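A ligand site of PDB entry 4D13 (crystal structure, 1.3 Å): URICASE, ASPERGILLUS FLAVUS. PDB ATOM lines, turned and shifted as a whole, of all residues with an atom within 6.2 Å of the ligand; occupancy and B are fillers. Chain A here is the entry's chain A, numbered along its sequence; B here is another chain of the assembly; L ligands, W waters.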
ATOM      1  N   GLN A 159      17.573  18.846  -8.704  1.00  0.00           N
ATOM      2  CA  GLN A 159      16.645  18.860  -7.589  1.00  0.00           C
ATOM      3  C   GLN A 159      17.410  18.764  -6.288  1.00  0.00           C
ATOM      4  O   GLN A 159      18.537  18.277  -6.254  1.00  0.00           O
ATOM      5  CB  GLN A 159      15.679  17.678  -7.709  1.00  0.00           C
ATOM      6  CG  GLN A 159      15.050  17.557  -9.076  1.00  0.00           C
ATOM      7  CD  GLN A 159      13.988  16.495  -9.153  1.00  0.00           C
ATOM      8  OE1 GLN A 159      13.226  16.295  -8.218  1.00  0.00           O
ATOM      9  NE2 GLN A 159      13.920  15.852 -10.281  1.00  0.00           N
ATOM     10  N   PHE A 160      16.764  19.182  -5.188  1.00  0.00           N
ATOM     11  CA  PHE A 160      17.332  18.913  -3.873  1.00  0.00           C
ATOM     12  C   PHE A 160      16.213  18.990  -2.836  1.00  0.00           C
ATOM     13  O   PHE A 160      15.777  20.073  -2.408  1.00  0.00           O
ATOM     14  CB  PHE A 160      18.492  19.857  -3.571  1.00  0.00           C
ATOM     15  CG  PHE A 160      19.291  19.456  -2.365  1.00  0.00           C
ATOM     16  CD1 PHE A 160      19.923  18.215  -2.326  1.00  0.00           C
ATOM     17  CD2 PHE A 160      19.397  20.263  -1.240  1.00  0.00           C
ATOM     18  CE1 PHE A 160      20.630  17.829  -1.214  1.00  0.00           C
ATOM     19  CE2 PHE A 160      20.109  19.883  -0.119  1.00  0.00           C
ATOM     20  CZ  PHE A 160      20.739  18.649  -0.109  1.00  0.00           C
ATOM     21  N   LEU A 171      16.588  26.167   4.450  1.00  0.00           N
ATOM     22  CA  LEU A 171      16.543  25.916   3.017  1.00  0.00           C
ATOM     23  C   LEU A 171      15.243  25.264   2.579  1.00  0.00           C
ATOM     24  O   LEU A 171      14.839  24.230   3.131  1.00  0.00           O
ATOM     25  CB  LEU A 171      17.713  24.995   2.620  1.00  0.00           C
ATOM     26  CG  LEU A 171      17.871  24.683   1.136  1.00  0.00           C
ATOM     27  CD1 LEU A 171      18.215  25.930   0.334  1.00  0.00           C
ATOM     28  CD2 LEU A 171      18.947  23.626   0.947  1.00  0.00           C
ATOM     29  N   ARG A 177      15.968  23.407  -9.977  1.00  0.00           N
ATOM     30  CA  ARG A 177      16.947  24.445  -9.678  1.00  0.00           C
ATOM     31  C   ARG A 177      18.058  24.413 -10.713  1.00  0.00           C
ATOM     32  O   ARG A 177      18.179  23.485 -11.506  1.00  0.00           O
ATOM     33  CB  ARG A 177      17.546  24.296  -8.274  1.00  0.00           C
ATOM     34  CG  ARG A 177      18.403  23.054  -8.133  1.00  0.00           C
ATOM     35  CD  ARG A 177      19.075  22.885  -6.812  1.00  0.00           C
ATOM     36  NE  ARG A 177      19.959  21.739  -6.826  1.00  0.00           N
ATOM     37  CZ  ARG A 177      20.789  21.398  -5.843  1.00  0.00           C
ATOM     38  NH1 ARG A 177      20.805  22.048  -4.684  1.00  0.00           N
ATOM     39  NH2 ARG A 177      21.640  20.375  -6.004  1.00  0.00           N
ATOM     40  N   LEU A 179      22.063  24.020 -11.426  1.00  0.00           N
ATOM     41  CA  LEU A 179      23.269  23.408 -10.868  1.00  0.00           C
ATOM     42  C   LEU A 179      24.464  23.840 -11.693  1.00  0.00           C
ATOM     43  O   LEU A 179      24.491  23.670 -12.907  1.00  0.00           O
ATOM     44  CB  LEU A 179      23.142  21.889 -10.855  1.00  0.00           C
ATOM     45  CG  LEU A 179      24.380  21.134 -10.363  1.00  0.00           C
ATOM     46  CD1 LEU A 179      24.735  21.529  -8.927  1.00  0.00           C
ATOM     47  CD2 LEU A 179      24.137  19.643 -10.478  1.00  0.00           C
ATOM     48  N   SER A 225      19.240  15.345 -11.573  1.00  0.00           N
ATOM     49  CA  SER A 225      20.084  15.156 -10.413  1.00  0.00           C
ATOM     50  C   SER A 225      19.331  15.260  -9.092  1.00  0.00           C
ATOM     51  O   SER A 225      18.659  16.261  -8.835  1.00  0.00           O
ATOM     52  CB  SER A 225      21.182  16.207 -10.433  1.00  0.00           C
ATOM     53  OG  SER A 225      21.962  16.194  -9.263  1.00  0.00           O
ATOM     54  N   ALA A 226      19.484  14.249  -8.237  1.00  0.00           N
ATOM     55  CA  ALA A 226      18.911  14.260  -6.889  1.00  0.00           C
ATOM     56  C   ALA A 226      19.738  15.070  -5.905  1.00  0.00           C
ATOM     57  O   ALA A 226      19.220  15.491  -4.862  1.00  0.00           O
ATOM     58  CB  ALA A 226      18.785  12.850  -6.383  1.00  0.00           C
ATOM     59  N   SER A 227      21.014  15.269  -6.242  1.00  0.00           N
ATOM     60  CA  SER A 227      21.976  15.983  -5.421  1.00  0.00           C
ATOM     61  C   SER A 227      23.299  15.950  -6.175  1.00  0.00           C
ATOM     62  O   SER A 227      23.496  15.093  -7.055  1.00  0.00           O
ATOM     63  CB  SER A 227      22.202  15.339  -4.057  1.00  0.00           C
ATOM     64  OG  SER A 227      22.776  14.059  -4.206  1.00  0.00           O
ATOM     65  N   VAL A 228      24.220  16.819  -5.787  1.00  0.00           N
ATOM     66  CA  VAL A 228      25.573  16.743  -6.305  1.00  0.00           C
ATOM     67  C   VAL A 228      26.193  15.374  -5.962  1.00  0.00           C
ATOM     68  O   VAL A 228      26.826  14.744  -6.807  1.00  0.00           O
ATOM     69  CB  VAL A 228      26.421  17.899  -5.758  1.00  0.00           C
ATOM     70  CG1 VAL A 228      27.873  17.769  -6.237  1.00  0.00           C
ATOM     71  CG2 VAL A 228      25.851  19.231  -6.213  1.00  0.00           C
ATOM     72  N   GLN A 229      25.975  14.941  -4.729  1.00  0.00           N
ATOM     73  CA  GLN A 229      26.451  13.644  -4.242  1.00  0.00           C
ATOM     74  C   GLN A 229      26.045  12.512  -5.194  1.00  0.00           C
ATOM     75  O   GLN A 229      26.885  11.684  -5.589  1.00  0.00           O
ATOM     76  CB  GLN A 229      25.856  13.371  -2.865  1.00  0.00           C
ATOM     77  CG  GLN A 229      26.417  14.200  -1.714  1.00  0.00           C
ATOM     78  CD  GLN A 229      25.752  15.559  -1.449  1.00  0.00           C
ATOM     79  OE1 GLN A 229      25.145  16.168  -2.340  1.00  0.00           O
ATOM     80  NE2 GLN A 229      25.900  16.052  -0.242  1.00  0.00           N
ATOM     81  N   ASN A 255      29.277  23.602  -5.180  1.00  0.00           N
ATOM     82  CA  ASN A 255      27.916  23.893  -5.605  1.00  0.00           C
ATOM     83  C   ASN A 255      27.830  25.418  -5.689  1.00  0.00           C
ATOM     84  O   ASN A 255      27.795  26.087  -4.656  1.00  0.00           O
ATOM     85  CB  ASN A 255      26.924  23.320  -4.610  1.00  0.00           C
ATOM     86  CG  ASN A 255      25.510  23.335  -5.134  1.00  0.00           C
ATOM     87  OD1 ASN A 255      25.237  23.735  -6.270  1.00  0.00           O
ATOM     88  ND2 ASN A 255      24.589  22.819  -4.316  1.00  0.00           N
ATOM     89  N   HIS A 257      26.115  28.462  -6.140  1.00  0.00           N
ATOM     90  CA  HIS A 257      24.680  28.693  -6.001  1.00  0.00           C
ATOM     91  C   HIS A 257      24.203  29.860  -6.845  1.00  0.00           C
ATOM     92  O   HIS A 257      24.875  30.886  -6.951  1.00  0.00           O
ATOM     93  CB  HIS A 257      24.325  28.968  -4.545  1.00  0.00           C
ATOM     94  CG  HIS A 257      24.814  27.899  -3.602  1.00  0.00           C
ATOM     95  ND1 HIS A 257      24.330  26.617  -3.588  1.00  0.00           N
ATOM     96  CD2 HIS A 257      25.770  27.944  -2.642  1.00  0.00           C
ATOM     97  CE1 HIS A 257      24.971  25.920  -2.659  1.00  0.00           C
ATOM     98  NE2 HIS A 257      25.843  26.706  -2.065  1.00  0.00           N
ATOM     99  N   ASN A 286      29.890  28.662  -0.838  1.00  0.00           N
ATOM    100  CA  ASN A 286      29.536  27.614  -1.776  1.00  0.00           C
ATOM    101  C   ASN A 286      29.561  26.277  -1.068  1.00  0.00           C
ATOM    102  O   ASN A 286      30.472  25.991  -0.289  1.00  0.00           O
ATOM    103  CB  ASN A 286      30.453  27.554  -3.020  1.00  0.00           C
ATOM    104  CG  ASN A 286      31.903  27.329  -2.673  1.00  0.00           C
ATOM    105  OD1 ASN A 286      32.597  28.278  -2.321  1.00  0.00           O
ATOM    106  ND2 ASN A 286      32.386  26.105  -2.815  1.00  0.00           N
ATOM    107  N   GLY A 287      28.600  25.420  -1.396  1.00  0.00           N
ATOM    108  CA  GLY A 287      28.732  24.030  -1.001  1.00  0.00           C
ATOM    109  C   GLY A 287      30.006  23.463  -1.605  1.00  0.00           C
ATOM    110  O   GLY A 287      30.464  23.885  -2.674  1.00  0.00           O
ATOM    111  N   LEU A 288      30.574  22.474  -0.929  1.00  0.00           N
ATOM    112  CA  LEU A 288      31.740  21.736  -1.433  1.00  0.00           C
ATOM    113  C   LEU A 288      31.506  20.292  -1.109  1.00  0.00           C
ATOM    114  O   LEU A 288      31.347  19.922   0.049  1.00  0.00           O
ATOM    115  CB  LEU A 288      33.022  22.263  -0.789  1.00  0.00           C
ATOM    116  CG  LEU A 288      34.292  21.545  -1.201  1.00  0.00           C
ATOM    117  CD1 LEU A 288      34.514  21.611  -2.702  1.00  0.00           C
ATOM    118  CD2 LEU A 288      35.516  22.130  -0.491  1.00  0.00           C
ATOM    119  N   ILE A 289      31.473  19.477  -2.163  1.00  0.00           N
ATOM    120  CA  ILE A 289      31.042  18.069  -2.059  1.00  0.00           C
ATOM    121  C   ILE A 289      32.178  17.204  -2.599  1.00  0.00           C
ATOM    122  O   ILE A 289      32.649  17.452  -3.720  1.00  0.00           O
ATOM    123  CB  ILE A 289      29.758  17.806  -2.872  1.00  0.00           C
ATOM    124  CG1 ILE A 289      28.720  18.958  -2.731  1.00  0.00           C
ATOM    125  CG2 ILE A 289      29.147  16.474  -2.475  1.00  0.00           C
ATOM    126  CD1 ILE A 289      28.178  19.164  -1.327  1.00  0.00           C
ATOM    127  N   TYR B   9      31.692  16.576   2.949  1.00  0.00           N
ATOM    128  CA  TYR B   9      30.951  17.623   2.266  1.00  0.00           C
ATOM    129  C   TYR B   9      30.596  18.710   3.265  1.00  0.00           C
ATOM    130  O   TYR B   9      30.507  18.470   4.476  1.00  0.00           O
ATOM    131  CB  TYR B   9      29.678  17.057   1.566  1.00  0.00           C
ATOM    132  CG  TYR B   9      28.547  16.976   2.565  1.00  0.00           C
ATOM    133  CD1 TYR B   9      28.521  16.007   3.560  1.00  0.00           C
ATOM    134  CD2 TYR B   9      27.575  17.955   2.593  1.00  0.00           C
ATOM    135  CE1 TYR B   9      27.557  16.034   4.559  1.00  0.00           C
ATOM    136  CE2 TYR B   9      26.615  17.986   3.576  1.00  0.00           C
ATOM    137  CZ  TYR B   9      26.613  17.035   4.575  1.00  0.00           C
ATOM    138  OH  TYR B   9      25.709  17.057   5.612  1.00  0.00           O
ATOM    139  N   GLY B  10      30.337  19.910   2.766  1.00  0.00           N
ATOM    140  CA  GLY B  10      29.926  20.998   3.653  1.00  0.00           C
ATOM    141  C   GLY B  10      29.939  22.326   2.959  1.00  0.00           C
ATOM    142  O   GLY B  10      29.759  22.393   1.744  1.00  0.00           O
ATOM    143  N   LYS B  11      30.101  23.398   3.742  1.00  0.00           N
ATOM    144  CA  LYS B  11      30.090  24.742   3.174  1.00  0.00           C
ATOM    145  C   LYS B  11      31.469  25.349   3.282  1.00  0.00           C
ATOM    146  O   LYS B  11      32.072  25.349   4.360  1.00  0.00           O
ATOM    147  CB  LYS B  11      29.077  25.641   3.851  1.00  0.00           C
ATOM    148  CG  LYS B  11      28.800  26.903   3.037  1.00  0.00           C
ATOM    149  CD  LYS B  11      27.934  26.669   1.814  1.00  0.00           C
ATOM    150  CE  LYS B  11      26.447  26.869   2.044  1.00  0.00           C
ATOM    151  NZ  LYS B  11      25.638  26.225   0.978  1.00  0.00           N
ATOM    152  N   ASN B  52      18.869  11.625   0.573  1.00  0.00           N
ATOM    153  CA  ASN B  52      19.206  12.916   1.151  1.00  0.00           C
ATOM    154  C   ASN B  52      18.924  13.031   2.645  1.00  0.00           C
ATOM    155  O   ASN B  52      19.306  14.009   3.264  1.00  0.00           O
ATOM    156  CB  ASN B  52      18.559  14.055   0.372  1.00  0.00           C
ATOM    157  CG  ASN B  52      19.179  14.248  -0.992  1.00  0.00           C
ATOM    158  OD1 ASN B  52      20.374  13.941  -1.181  1.00  0.00           O
ATOM    159  ND2 ASN B  52      18.401  14.773  -1.946  1.00  0.00           N
ATOM    160  N   ILE B  55      21.796  13.945   4.814  1.00  0.00           N
ATOM    161  CA  ILE B  55      22.497  15.187   4.543  1.00  0.00           C
ATOM    162  C   ILE B  55      21.952  16.312   5.416  1.00  0.00           C
ATOM    163  O   ILE B  55      20.781  16.721   5.310  1.00  0.00           O
ATOM    164  CB  ILE B  55      22.437  15.556   3.059  1.00  0.00           C
ATOM    165  CG1 ILE B  55      23.176  14.486   2.230  1.00  0.00           C
ATOM    166  CG2 ILE B  55      23.014  16.951   2.838  1.00  0.00           C
ATOM    167  CD1 ILE B  55      24.627  14.253   2.606  1.00  0.00           C
ATOM    168  N   VAL B  56      22.838  16.811   6.286  1.00  0.00           N
ATOM    169  CA  VAL B  56      22.678  18.125   6.892  1.00  0.00           C
ATOM    170  C   VAL B  56      23.043  19.143   5.795  1.00  0.00           C
ATOM    171  O   VAL B  56      24.179  19.177   5.318  1.00  0.00           O
ATOM    172  CB  VAL B  56      23.599  18.282   8.124  1.00  0.00           C
ATOM    173  CG1 VAL B  56      23.509  19.673   8.704  1.00  0.00           C
ATOM    174  CG2 VAL B  56      23.281  17.238   9.179  1.00  0.00           C
ATOM    175  N   ALA B  57      22.057  19.886   5.287  1.00  0.00           N
ATOM    176  CA  ALA B  57      22.291  20.711   4.101  1.00  0.00           C
ATOM    177  C   ALA B  57      23.460  21.637   4.322  1.00  0.00           C
ATOM    178  O   ALA B  57      23.627  22.209   5.412  1.00  0.00           O
ATOM    179  CB  ALA B  57      21.040  21.518   3.756  1.00  0.00           C
ATOM    180  N   THR B  58      24.243  21.886   3.275  1.00  0.00           N
ATOM    181  CA  THR B  58      25.325  22.848   3.439  1.00  0.00           C
ATOM    182  C   THR B  58      24.791  24.228   3.833  1.00  0.00           C
ATOM    183  O   THR B  58      25.442  24.956   4.608  1.00  0.00           O
ATOM    184  CB  THR B  58      26.258  22.919   2.221  1.00  0.00           C
ATOM    185  OG1 THR B  58      25.614  23.562   1.103  1.00  0.00           O
ATOM    186  CG2 THR B  58      26.725  21.536   1.821  1.00  0.00           C
ATOM    187  N   ASP B  59      23.593  24.584   3.349  1.00  0.00           N
ATOM    188  CA  ASP B  59      22.967  25.836   3.747  1.00  0.00           C
ATOM    189  C   ASP B  59      22.776  25.873   5.260  1.00  0.00           C
ATOM    190  O   ASP B  59      22.919  26.921   5.893  1.00  0.00           O
ATOM    191  CB  ASP B  59      21.629  25.989   3.047  1.00  0.00           C
ATOM    192  CG  ASP B  59      21.037  27.360   3.224  1.00  0.00           C
ATOM    193  OD1 ASP B  59      21.495  28.291   2.522  1.00  0.00           O
ATOM    194  OD2 ASP B  59      20.146  27.504   4.097  1.00  0.00           O
ATOM    195  N   SER B  60      22.358  24.738   5.842  1.00  0.00           N
ATOM    196  CA  SER B  60      22.221  24.636   7.290  1.00  0.00           C
ATOM    197  C   SER B  60      23.543  24.719   8.031  1.00  0.00           C
ATOM    198  O   SER B  60      23.605  25.276   9.127  1.00  0.00           O
ATOM    199  CB  SER B  60      21.477  23.342   7.673  1.00  0.00           C
ATOM    200  OG  SER B  60      20.241  23.254   6.960  1.00  0.00           O
HETATM  201  N1  LIG L   1      23.875  18.804  -1.899  1.00  0.00           N
HETATM  202  C1  LIG L   1      23.259  19.477  -2.949  1.00  0.00           C
HETATM  203  C2  LIG L   1      24.106  19.302  -0.644  1.00  0.00           C
HETATM  204  N2  LIG L   1      22.683  20.714  -2.773  1.00  0.00           N
HETATM  205  O1  LIG L   1      23.215  18.928  -4.056  1.00  0.00           O
HETATM  206  C3  LIG L   1      22.890  21.283  -1.613  1.00  0.00           C
HETATM  207  C4  LIG L   1      23.846  20.790  -0.569  1.00  0.00           C
HETATM  208  N3  LIG L   1      22.304  22.346  -1.045  1.00  0.00           N
HETATM  209  O2  LIG L   1      24.539  18.623   0.278  1.00  0.00           O
HETATM  210  N4  LIG L   1      23.524  21.412   0.667  1.00  0.00           N
HETATM  211  C5  LIG L   1      22.681  22.410   0.293  1.00  0.00           C
HETATM  212  O3  LIG L   1      22.314  23.349   1.013  1.00  0.00           O
HETATM  213  O4  LIG L   1      25.205  21.164  -1.121  1.00  0.00           O
HETATM  214  O5  LIG L   1      25.419  22.604  -1.335  1.00  0.00           O
HETATM  215  O   HOH W   1      21.075  24.481  -2.459  1.00  0.00           O
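N of Thr 58 of chain B sits at hydrogen-bond distance from O3 of the ligand (3.3 Å).
The side-chain hydroxyl (OG1) of Thr 58 of chain B sits at hydrogen-bond distance from an oxygen (O5) of the ligand.
O1 of the ligand sits at hydrogen-bond distance from NH2 of Arg 177, at 2.9 Å.
The backbone NH (N) of Val 228 is in hydrogen-bond range of an oxygen (O1) of the ligand (2.9 Å).
O3 of the ligand sits at hydrogen-bond distance from N of Asp 59 of chain B (2.9 Å).
NE2 of Gln 229 sits at hydrogen-bond distance from O2 of the ligand, 3.0 Å away.
The side-chain amide nitrogen (ND2) of Asn 255 lies within hydrogen-bond range of an oxygen (O5) of the ligand (3.1 Å).
The side-chain amino group (NZ) of Lys 11 of chain B sits at hydrogen-bond distance from the side-chain hydroxyl (OG1) of Thr 58 of chain B, at 2.7 Å.
OG of Ser 227 lies close to N of Gln 229, at 3.4 Å.
O of Asn 255 is in hydrogen-bond range of NE2 of His 257.
N of Asn 255 sits at hydrogen-bond distance from O of Gly 287, 2.8 Å away.
The backbone carbonyl oxygen of Ser 227 is in hydrogen-bond range of the side-chain hydroxyl of Ser 225 (2.9 Å).
A ring nitrogen (NE2) of His 257 sits at hydrogen-bond distance from the backbone NH (N) of Gly 287 (3.1 Å).
NZ of Lys 11 of chain B is in hydrogen-bond range of NE2 of His 257.
The backbone carbonyl oxygen of Val 56 of chain B lies within hydrogen-bond range of the side-chain hydroxyl of Tyr 9 of chain B.
Water W1 lies within hydrogen-bond range of a nitrogen (N3) of the ligand (2.8 Å) and the guanidinium group of Arg 177 (3.3 Å).
CE2 of Phe 160 touches N3 of the ligand, at 3.4 Å.
Leu 171 touches the ligand.
Ser 227 touches the ligand (CA to O1, 3.5 Å).
His 257 touches the ligand.
CA of Gly 287 touches O5 of the ligand (3.6 Å).
Ile 289 touches the ligand.
Tyr 9 of chain B touches the ligand.
CG2 of Ile 55 of chain B touches O2 of the ligand (3.4 Å).
CB of Ala 57 of chain B touches O3 of the ligand (3.5 Å).
15 residues have an atom within 4 Å of the ligand: Phe 160, Leu 171, Arg 177, Ser 227, Val 228, Gln 229, Asn 255, His 257, Gly 287, Ile 289, Tyr 9 of chain B, Ile 55 of chain B, Ala 57 of chain B, Thr 58 of chain B and Asp 59 of chain B.
The nearest printed residue that does not touch the ligand is Lys 11 of chain B (4.3 Å).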
